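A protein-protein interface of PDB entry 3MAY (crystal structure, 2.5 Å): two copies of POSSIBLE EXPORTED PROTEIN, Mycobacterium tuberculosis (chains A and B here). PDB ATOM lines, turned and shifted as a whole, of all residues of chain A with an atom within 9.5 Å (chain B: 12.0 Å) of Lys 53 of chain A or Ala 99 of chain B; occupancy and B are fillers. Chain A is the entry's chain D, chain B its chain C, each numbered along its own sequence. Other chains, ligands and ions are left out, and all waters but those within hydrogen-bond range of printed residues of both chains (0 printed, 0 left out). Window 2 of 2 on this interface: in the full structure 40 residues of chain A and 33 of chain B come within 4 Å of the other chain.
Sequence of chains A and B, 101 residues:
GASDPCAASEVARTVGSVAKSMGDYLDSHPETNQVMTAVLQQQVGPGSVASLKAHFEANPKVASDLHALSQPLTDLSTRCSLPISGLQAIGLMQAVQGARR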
ATOM      1  N   VAL A  35      24.142 -11.498 -20.776  1.00  0.00           N
ATOM      2  CA  VAL A  35      25.049 -10.831 -21.686  1.00  0.00           C
ATOM      3  C   VAL A  35      26.463 -10.941 -21.076  1.00  0.00           C
ATOM      4  O   VAL A  35      27.436 -11.388 -21.780  1.00  0.00           O
ATOM      5  CB  VAL A  35      24.648  -9.355 -21.879  1.00  0.00           C
ATOM      6  CG1 VAL A  35      25.819  -8.501 -22.480  1.00  0.00           C
ATOM      7  CG2 VAL A  35      23.391  -9.227 -22.756  1.00  0.00           C
ATOM      8  N   MET A  36      26.591 -10.606 -19.779  1.00  0.00           N
ATOM      9  CA  MET A  36      27.910 -10.645 -19.110  1.00  0.00           C
ATOM     10  C   MET A  36      28.453 -12.045 -19.089  1.00  0.00           C
ATOM     11  O   MET A  36      29.627 -12.274 -19.297  1.00  0.00           O
ATOM     12  CB  MET A  36      27.870 -10.092 -17.696  1.00  0.00           C
ATOM     13  CG  MET A  36      27.303  -8.645 -17.590  1.00  0.00           C
ATOM     14  SD  MET A  36      28.615  -7.477 -17.952  1.00  0.00           S
ATOM     15  CE  MET A  36      27.674  -5.945 -18.110  1.00  0.00           C
ATOM     16  N   VAL A  39      29.990 -12.953 -22.345  1.00  0.00           N
ATOM     17  CA  VAL A  39      31.290 -12.340 -22.524  1.00  0.00           C
ATOM     18  C   VAL A  39      32.414 -13.137 -21.835  1.00  0.00           C
ATOM     19  O   VAL A  39      33.393 -13.463 -22.492  1.00  0.00           O
ATOM     20  CB  VAL A  39      31.324 -10.863 -22.107  1.00  0.00           C
ATOM     21  CG1 VAL A  39      32.805 -10.344 -22.133  1.00  0.00           C
ATOM     22  CG2 VAL A  39      30.449 -10.088 -23.024  1.00  0.00           C
ATOM     23  N   GLY A  47      33.960  -9.293 -30.397  1.00  0.00           N
ATOM     24  CA  GLY A  47      32.953  -8.262 -30.163  1.00  0.00           C
ATOM     25  C   GLY A  47      32.352  -8.436 -28.770  1.00  0.00           C
ATOM     26  O   GLY A  47      31.148  -8.537 -28.636  1.00  0.00           O
ATOM     27  N   SER A  48      33.193  -8.532 -27.746  1.00  0.00           N
ATOM     28  CA  SER A  48      32.682  -8.577 -26.403  1.00  0.00           C
ATOM     29  C   SER A  48      32.442  -7.119 -25.999  1.00  0.00           C
ATOM     30  O   SER A  48      31.440  -6.805 -25.363  1.00  0.00           O
ATOM     31  CB  SER A  48      33.541  -9.466 -25.445  1.00  0.00           C
ATOM     32  OG  SER A  48      34.645  -8.802 -24.870  1.00  0.00           O
ATOM     33  N   VAL A  49      33.303  -6.217 -26.458  1.00  0.00           N
ATOM     34  CA  VAL A  49      32.996  -4.775 -26.397  1.00  0.00           C
ATOM     35  C   VAL A  49      31.736  -4.439 -27.199  1.00  0.00           C
ATOM     36  O   VAL A  49      30.891  -3.686 -26.736  1.00  0.00           O
ATOM     37  CB  VAL A  49      34.171  -3.897 -26.895  1.00  0.00           C
ATOM     38  CG1 VAL A  49      33.666  -2.548 -27.470  1.00  0.00           C
ATOM     39  CG2 VAL A  49      35.204  -3.665 -25.785  1.00  0.00           C
ATOM     40  N   ALA A  50      31.620  -5.021 -28.391  1.00  0.00           N
ATOM     41  CA  ALA A  50      30.547  -4.671 -29.292  1.00  0.00           C
ATOM     42  C   ALA A  50      29.219  -5.149 -28.740  1.00  0.00           C
ATOM     43  O   ALA A  50      28.249  -4.395 -28.733  1.00  0.00           O
ATOM     44  CB  ALA A  50      30.803  -5.192 -30.742  1.00  0.00           C
ATOM     45  N   SER A  51      29.155  -6.374 -28.251  1.00  0.00           N
ATOM     46  CA  SER A  51      27.867  -6.850 -27.789  1.00  0.00           C
ATOM     47  C   SER A  51      27.447  -6.117 -26.520  1.00  0.00           C
ATOM     48  O   SER A  51      26.265  -6.116 -26.194  1.00  0.00           O
ATOM     49  CB  SER A  51      27.865  -8.340 -27.537  1.00  0.00           C
ATOM     50  OG  SER A  51      28.785  -8.648 -26.523  1.00  0.00           O
ATOM     51  N   LEU A  52      28.421  -5.507 -25.830  1.00  0.00           N
ATOM     52  CA  LEU A  52      28.175  -4.786 -24.608  1.00  0.00           C
ATOM     53  C   LEU A  52      27.511  -3.474 -24.954  1.00  0.00           C
ATOM     54  O   LEU A  52      26.482  -3.115 -24.314  1.00  0.00           O
ATOM     55  CB  LEU A  52      29.449  -4.575 -23.768  1.00  0.00           C
ATOM     56  CG  LEU A  52      29.887  -5.697 -22.769  1.00  0.00           C
ATOM     57  CD1 LEU A  52      31.173  -5.346 -21.999  1.00  0.00           C
ATOM     58  CD2 LEU A  52      28.840  -6.033 -21.755  1.00  0.00           C
ATOM     59  N   LYS A  53      28.052  -2.786 -25.984  1.00  0.00           N
ATOM     60  CA  LYS A  53      27.455  -1.554 -26.480  1.00  0.00           C
ATOM     61  C   LYS A  53      26.020  -1.810 -26.942  1.00  0.00           C
ATOM     62  O   LYS A  53      25.141  -0.973 -26.702  1.00  0.00           O
ATOM     63  CB  LYS A  53      28.263  -0.947 -27.655  1.00  0.00           C
ATOM     64  CG  LYS A  53      29.211   0.224 -27.296  1.00  0.00           C
ATOM     65  CD  LYS A  53      29.166   1.377 -28.317  1.00  0.00           C
ATOM     66  CE  LYS A  53      30.449   2.277 -28.198  1.00  0.00           C
ATOM     67  NZ  LYS A  53      30.239   3.780 -28.193  1.00  0.00           N
ATOM     68  N   ALA A  54      25.797  -2.945 -27.620  1.00  0.00           N
ATOM     69  CA  ALA A  54      24.495  -3.229 -28.211  1.00  0.00           C
ATOM     70  C   ALA A  54      23.491  -3.389 -27.085  1.00  0.00           C
ATOM     71  O   ALA A  54      22.328  -2.984 -27.183  1.00  0.00           O
ATOM     72  CB  ALA A  54      24.546  -4.455 -29.054  1.00  0.00           C
ATOM     73  N   HIS A  55      23.962  -3.919 -25.978  1.00  0.00           N
ATOM     74  CA  HIS A  55      23.083  -4.127 -24.866  1.00  0.00           C
ATOM     75  C   HIS A  55      22.821  -2.835 -24.057  1.00  0.00           C
ATOM     76  O   HIS A  55      21.729  -2.670 -23.494  1.00  0.00           O
ATOM     77  CB  HIS A  55      23.621  -5.205 -23.969  1.00  0.00           C
ATOM     78  CG  HIS A  55      22.657  -5.598 -22.905  1.00  0.00           C
ATOM     79  ND1 HIS A  55      22.790  -5.185 -21.601  1.00  0.00           N
ATOM     80  CD2 HIS A  55      21.503  -6.311 -22.959  1.00  0.00           C
ATOM     81  CE1 HIS A  55      21.777  -5.649 -20.889  1.00  0.00           C
ATOM     82  NE2 HIS A  55      20.993  -6.349 -21.688  1.00  0.00           N
ATOM     83  N   PHE A  56      23.825  -1.957 -23.995  1.00  0.00           N
ATOM     84  CA  PHE A  56      23.734  -0.688 -23.310  1.00  0.00           C
ATOM     85  C   PHE A  56      22.923   0.368 -24.089  1.00  0.00           C
ATOM     86  O   PHE A  56      22.498   1.350 -23.483  1.00  0.00           O
ATOM     87  CB  PHE A  56      25.116  -0.103 -23.075  1.00  0.00           C
ATOM     88  CG  PHE A  56      25.910  -0.774 -21.974  1.00  0.00           C
ATOM     89  CD1 PHE A  56      25.448  -1.916 -21.333  1.00  0.00           C
ATOM     90  CD2 PHE A  56      27.144  -0.256 -21.608  1.00  0.00           C
ATOM     91  CE1 PHE A  56      26.185  -2.537 -20.342  1.00  0.00           C
ATOM     92  CE2 PHE A  56      27.885  -0.851 -20.639  1.00  0.00           C
ATOM     93  CZ  PHE A  56      27.397  -2.012 -19.981  1.00  0.00           C
ATOM     94  N   GLU A  57      22.764   0.190 -25.411  1.00  0.00           N
ATOM     95  CA  GLU A  57      22.063   1.158 -26.253  1.00  0.00           C
ATOM     96  C   GLU A  57      20.581   0.908 -26.096  1.00  0.00           C
ATOM     97  O   GLU A  57      19.737   1.821 -26.265  1.00  0.00           O
ATOM     98  CB  GLU A  57      22.427   1.008 -27.751  1.00  0.00           C
ATOM     99  CG  GLU A  57      23.722   1.696 -28.243  1.00  0.00           C
ATOM    100  CD  GLU A  57      24.097   1.241 -29.694  1.00  0.00           C
ATOM    101  OE1 GLU A  57      24.124  -0.005 -29.938  1.00  0.00           O
ATOM    102  OE2 GLU A  57      24.341   2.124 -30.581  1.00  0.00           O
ATOM    103  N   ALA A  58      20.287  -0.351 -25.801  1.00  0.00           N
ATOM    104  CA  ALA A  58      18.931  -0.826 -25.653  1.00  0.00           C
ATOM    105  C   ALA A  58      18.522  -0.648 -24.199  1.00  0.00           C
ATOM    106  O   ALA A  58      17.317  -0.545 -23.898  1.00  0.00           O
ATOM    107  CB  ALA A  58      18.876  -2.286 -26.048  1.00  0.00           C
ATOM    108  N   ASN A  59      19.541  -0.614 -23.322  1.00  0.00           N
ATOM    109  CA  ASN A  59      19.365  -0.549 -21.888  1.00  0.00           C
ATOM    110  C   ASN A  59      20.242   0.520 -21.206  1.00  0.00           C
ATOM    111  O   ASN A  59      21.185   0.181 -20.479  1.00  0.00           O
ATOM    112  CB  ASN A  59      19.637  -1.928 -21.284  1.00  0.00           C
ATOM    113  CG  ASN A  59      18.748  -3.040 -21.900  1.00  0.00           C
ATOM    114  OD1 ASN A  59      17.586  -3.201 -21.516  1.00  0.00           O
ATOM    115  ND2 ASN A  59      19.298  -3.779 -22.880  1.00  0.00           N
ATOM    116  N   PRO A  60      19.943   1.820 -21.445  1.00  0.00           N
ATOM    117  CA  PRO A  60      20.574   2.924 -20.764  1.00  0.00           C
ATOM    118  C   PRO A  60      20.457   2.909 -19.231  1.00  0.00           C
ATOM    119  O   PRO A  60      21.384   3.383 -18.534  1.00  0.00           O
ATOM    120  CB  PRO A  60      19.831   4.134 -21.338  1.00  0.00           C
ATOM    121  CG  PRO A  60      18.635   3.555 -22.061  1.00  0.00           C
ATOM    122  CD  PRO A  60      19.159   2.312 -22.590  1.00  0.00           C
ATOM    123  N   ALA A  63      22.971   0.513 -18.105  1.00  0.00           N
ATOM    124  CA  ALA A  63      24.307   1.116 -18.317  1.00  0.00           C
ATOM    125  C   ALA A  63      24.575   2.047 -17.140  1.00  0.00           C
ATOM    126  O   ALA A  63      25.611   1.979 -16.484  1.00  0.00           O
ATOM    127  CB  ALA A  63      24.415   1.893 -19.643  1.00  0.00           C
ATOM    128  N   HIS A  67      27.514   1.897 -13.868  1.00  0.00           N
ATOM    129  CA  HIS A  67      28.453   2.983 -13.657  1.00  0.00           C
ATOM    130  C   HIS A  67      28.378   3.456 -12.199  1.00  0.00           C
ATOM    131  O   HIS A  67      29.420   3.673 -11.550  1.00  0.00           O
ATOM    132  CB  HIS A  67      28.115   4.136 -14.620  1.00  0.00           C
ATOM    133  CG  HIS A  67      29.172   5.212 -14.727  1.00  0.00           C
ATOM    134  ND1 HIS A  67      30.291   5.085 -15.527  1.00  0.00           N
ATOM    135  CD2 HIS A  67      29.253   6.449 -14.175  1.00  0.00           C
ATOM    136  CE1 HIS A  67      31.017   6.186 -15.454  1.00  0.00           C
ATOM    137  NE2 HIS A  67      30.408   7.028 -14.643  1.00  0.00           N
ATOM    138  N   ILE B  90      38.822  -8.072 -14.364  1.00  0.00           N
ATOM    139  CA  ILE B  90      39.278  -6.717 -14.660  1.00  0.00           C
ATOM    140  C   ILE B  90      39.134  -6.415 -16.152  1.00  0.00           C
ATOM    141  O   ILE B  90      38.721  -5.312 -16.551  1.00  0.00           O
ATOM    142  CB  ILE B  90      40.694  -6.446 -14.126  1.00  0.00           C
ATOM    143  CG1 ILE B  90      40.633  -6.160 -12.623  1.00  0.00           C
ATOM    144  CG2 ILE B  90      41.319  -5.261 -14.866  1.00  0.00           C
ATOM    145  CD1 ILE B  90      41.930  -5.762 -12.024  1.00  0.00           C
ATOM    146  N   GLY B  91      39.460  -7.413 -16.972  1.00  0.00           N
ATOM    147  CA  GLY B  91      39.224  -7.350 -18.411  1.00  0.00           C
ATOM    148  C   GLY B  91      37.816  -6.880 -18.744  1.00  0.00           C
ATOM    149  O   GLY B  91      37.627  -5.885 -19.455  1.00  0.00           O
ATOM    150  N   LEU B  92      36.825  -7.597 -18.221  1.00  0.00           N
ATOM    151  CA  LEU B  92      35.417  -7.273 -18.449  1.00  0.00           C
ATOM    152  C   LEU B  92      35.014  -5.871 -17.970  1.00  0.00           C
ATOM    153  O   LEU B  92      34.168  -5.222 -18.585  1.00  0.00           O
ATOM    154  CB  LEU B  92      34.520  -8.329 -17.801  1.00  0.00           C
ATOM    155  CG  LEU B  92      33.012  -8.104 -17.614  1.00  0.00           C
ATOM    156  CD1 LEU B  92      32.263  -8.257 -18.875  1.00  0.00           C
ATOM    157  CD2 LEU B  92      32.501  -9.120 -16.599  1.00  0.00           C
ATOM    158  N   MET B  93      35.601  -5.427 -16.859  1.00  0.00           N
ATOM    159  CA  MET B  93      35.336  -4.081 -16.355  1.00  0.00           C
ATOM    160  C   MET B  93      35.827  -3.081 -17.397  1.00  0.00           C
ATOM    161  O   MET B  93      35.037  -2.273 -17.925  1.00  0.00           O
ATOM    162  CB  MET B  93      35.998  -3.862 -15.000  1.00  0.00           C
ATOM    163  CG  MET B  93      35.147  -3.063 -14.050  1.00  0.00           C
ATOM    164  SD  MET B  93      36.117  -2.184 -12.800  1.00  0.00           S
ATOM    165  CE  MET B  93      36.441  -0.646 -13.669  1.00  0.00           C
ATOM    166  N   GLN B  94      37.113  -3.188 -17.737  1.00  0.00           N
ATOM    167  CA  GLN B  94      37.701  -2.379 -18.821  1.00  0.00           C
ATOM    168  C   GLN B  94      36.850  -2.434 -20.054  1.00  0.00           C
ATOM    169  O   GLN B  94      36.703  -1.411 -20.726  1.00  0.00           O
ATOM    170  CB  GLN B  94      39.137  -2.778 -19.168  1.00  0.00           C
ATOM    171  CG  GLN B  94      40.108  -2.767 -17.970  1.00  0.00           C
ATOM    172  CD  GLN B  94      41.498  -3.281 -18.351  1.00  0.00           C
ATOM    173  OE1 GLN B  94      41.661  -4.056 -19.322  1.00  0.00           O
ATOM    174  NE2 GLN B  94      42.512  -2.853 -17.593  1.00  0.00           N
ATOM    175  N   ALA B  95      36.274  -3.601 -20.351  1.00  0.00           N
ATOM    176  CA  ALA B  95      35.396  -3.757 -21.537  1.00  0.00           C
ATOM    177  C   ALA B  95      34.102  -2.894 -21.496  1.00  0.00           C
ATOM    178  O   ALA B  95      33.708  -2.274 -22.510  1.00  0.00           O
ATOM    179  CB  ALA B  95      35.060  -5.249 -21.774  1.00  0.00           C
ATOM    180  N   VAL B  96      33.454  -2.873 -20.320  1.00  0.00           N
ATOM    181  CA  VAL B  96      32.359  -1.962 -20.030  1.00  0.00           C
ATOM    182  C   VAL B  96      32.793  -0.468 -20.200  1.00  0.00           C
ATOM    183  O   VAL B  96      32.190   0.260 -21.051  1.00  0.00           O
ATOM    184  CB  VAL B  96      31.739  -2.159 -18.623  1.00  0.00           C
ATOM    185  CG1 VAL B  96      30.541  -1.186 -18.428  1.00  0.00           C
ATOM    186  CG2 VAL B  96      31.337  -3.621 -18.369  1.00  0.00           C
ATOM    187  N   GLN B  97      33.810  -0.023 -19.433  1.00  0.00           N
ATOM    188  CA  GLN B  97      34.306   1.362 -19.534  1.00  0.00           C
ATOM    189  C   GLN B  97      34.459   1.693 -21.001  1.00  0.00           C
ATOM    190  O   GLN B  97      33.739   2.550 -21.471  1.00  0.00           O
ATOM    191  CB  GLN B  97      35.634   1.603 -18.769  1.00  0.00           C
ATOM    192  CG  GLN B  97      35.539   1.372 -17.270  1.00  0.00           C
ATOM    193  CD  GLN B  97      36.888   1.461 -16.498  1.00  0.00           C
ATOM    194  OE1 GLN B  97      37.938   0.898 -16.909  1.00  0.00           O
ATOM    195  NE2 GLN B  97      36.835   2.121 -15.326  1.00  0.00           N
ATOM    196  N   GLY B  98      35.306   0.971 -21.740  1.00  0.00           N
ATOM    197  CA  GLY B  98      35.460   1.203 -23.203  1.00  0.00           C
ATOM    198  C   GLY B  98      34.156   1.304 -23.984  1.00  0.00           C
ATOM    199  O   GLY B  98      34.081   2.023 -25.011  1.00  0.00           O
ATOM    200  N   ALA B  99      33.119   0.593 -23.526  1.00  0.00           N
ATOM    201  CA  ALA B  99      31.797   0.635 -24.217  1.00  0.00           C
ATOM    202  C   ALA B  99      31.050   1.943 -23.881  1.00  0.00           C
ATOM    203  O   ALA B  99      30.372   2.561 -24.741  1.00  0.00           O
ATOM    204  CB  ALA B  99      30.978  -0.566 -23.826  1.00  0.00           C
ATOM    205  N   ARG B 100      31.201   2.330 -22.606  1.00  0.00           N
ATOM    206  CA  ARG B 100      30.712   3.581 -22.049  1.00  0.00           C
ATOM    207  C   ARG B 100      31.298   4.755 -22.795  1.00  0.00           C
ATOM    208  O   ARG B 100      30.587   5.434 -23.570  1.00  0.00           O
ATOM    209  CB  ARG B 100      31.113   3.639 -20.557  1.00  0.00           C
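No position is printed for both chains. Of the 7 pairs that touch across the chains among the printed residues, none has its exchanged pair printed and touching as well.
Of the printed residues of chain B, Val 39 of chain A touches Leu 92 (3.9 Å). Of chain B, only Ala 95 comes within 4 Å of Val 49 of chain A. Ser 51 of chain A touches none of the printed residues of chain B. Leu 52 of chain A touches just these residues of chain B: Ala 95 (3.9 Å) and Val 96 (3.8 Å). Lys 53 of chain A touches one residue of chain B. Ala 54 of chain A touches none of the printed residues of chain B. Of the printed residues of chain B, Phe 56 of chain A touches Val 96. No residue of chain B comes within 4 Å of Glu 57 of chain A. Printed residues of chain A within 4 Å of Ala 95 of chain B: Val 49 and Leu 52. Of the printed residues of chain A, Val 96 of chain B touches Leu 52 and Phe 56. Gly 98 of chain B touches none of the printed residues of chain A. Ala 99 of chain B touches one residue of chain A. The nearest residue of chain B that does not touch Lys 53 of chain A is Gly 98 of chain B (4.8 Å). The nearest printed residue of chain A that does not touch Ala 99 of chain B is Val 49 of chain A (4.3 Å). The nearest printed residue of chain B that does not touch Val 39 of chain A is Ala 95 of chain B (5.6 Å).
Hydrophobic or aromatic side chains of chain A within 4 Å of the printed part of chain B: Met 36, Val 39, Val 49, Leu 52 and Phe 56. Among the printed residues, 7 pairs touch across the chains. Among the printed residues, no Asp or Glu carboxylate lies within 4 Å of a Lys or Arg side-chain nitrogen of the other chain.
Among the printed residues, pairs that only touch across the chains: Met 36 of chain A with Leu 92 of chain B (3.8 Å), Val 39 of chain A with Leu 92 of chain B (3.9 Å), Val 49 of chain A with Ala 95 of chain B (3.9 Å), Leu 52 of chain A with Ala 95 of chain B (3.9 Å), Leu 52 of chain A with Val 96 of chain B (3.8 Å), Lys 53 of chain A with Ala 99 of chain B (3.5 Å) and Phe 56 of chain A with Val 96 of chain B (3.5 Å).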
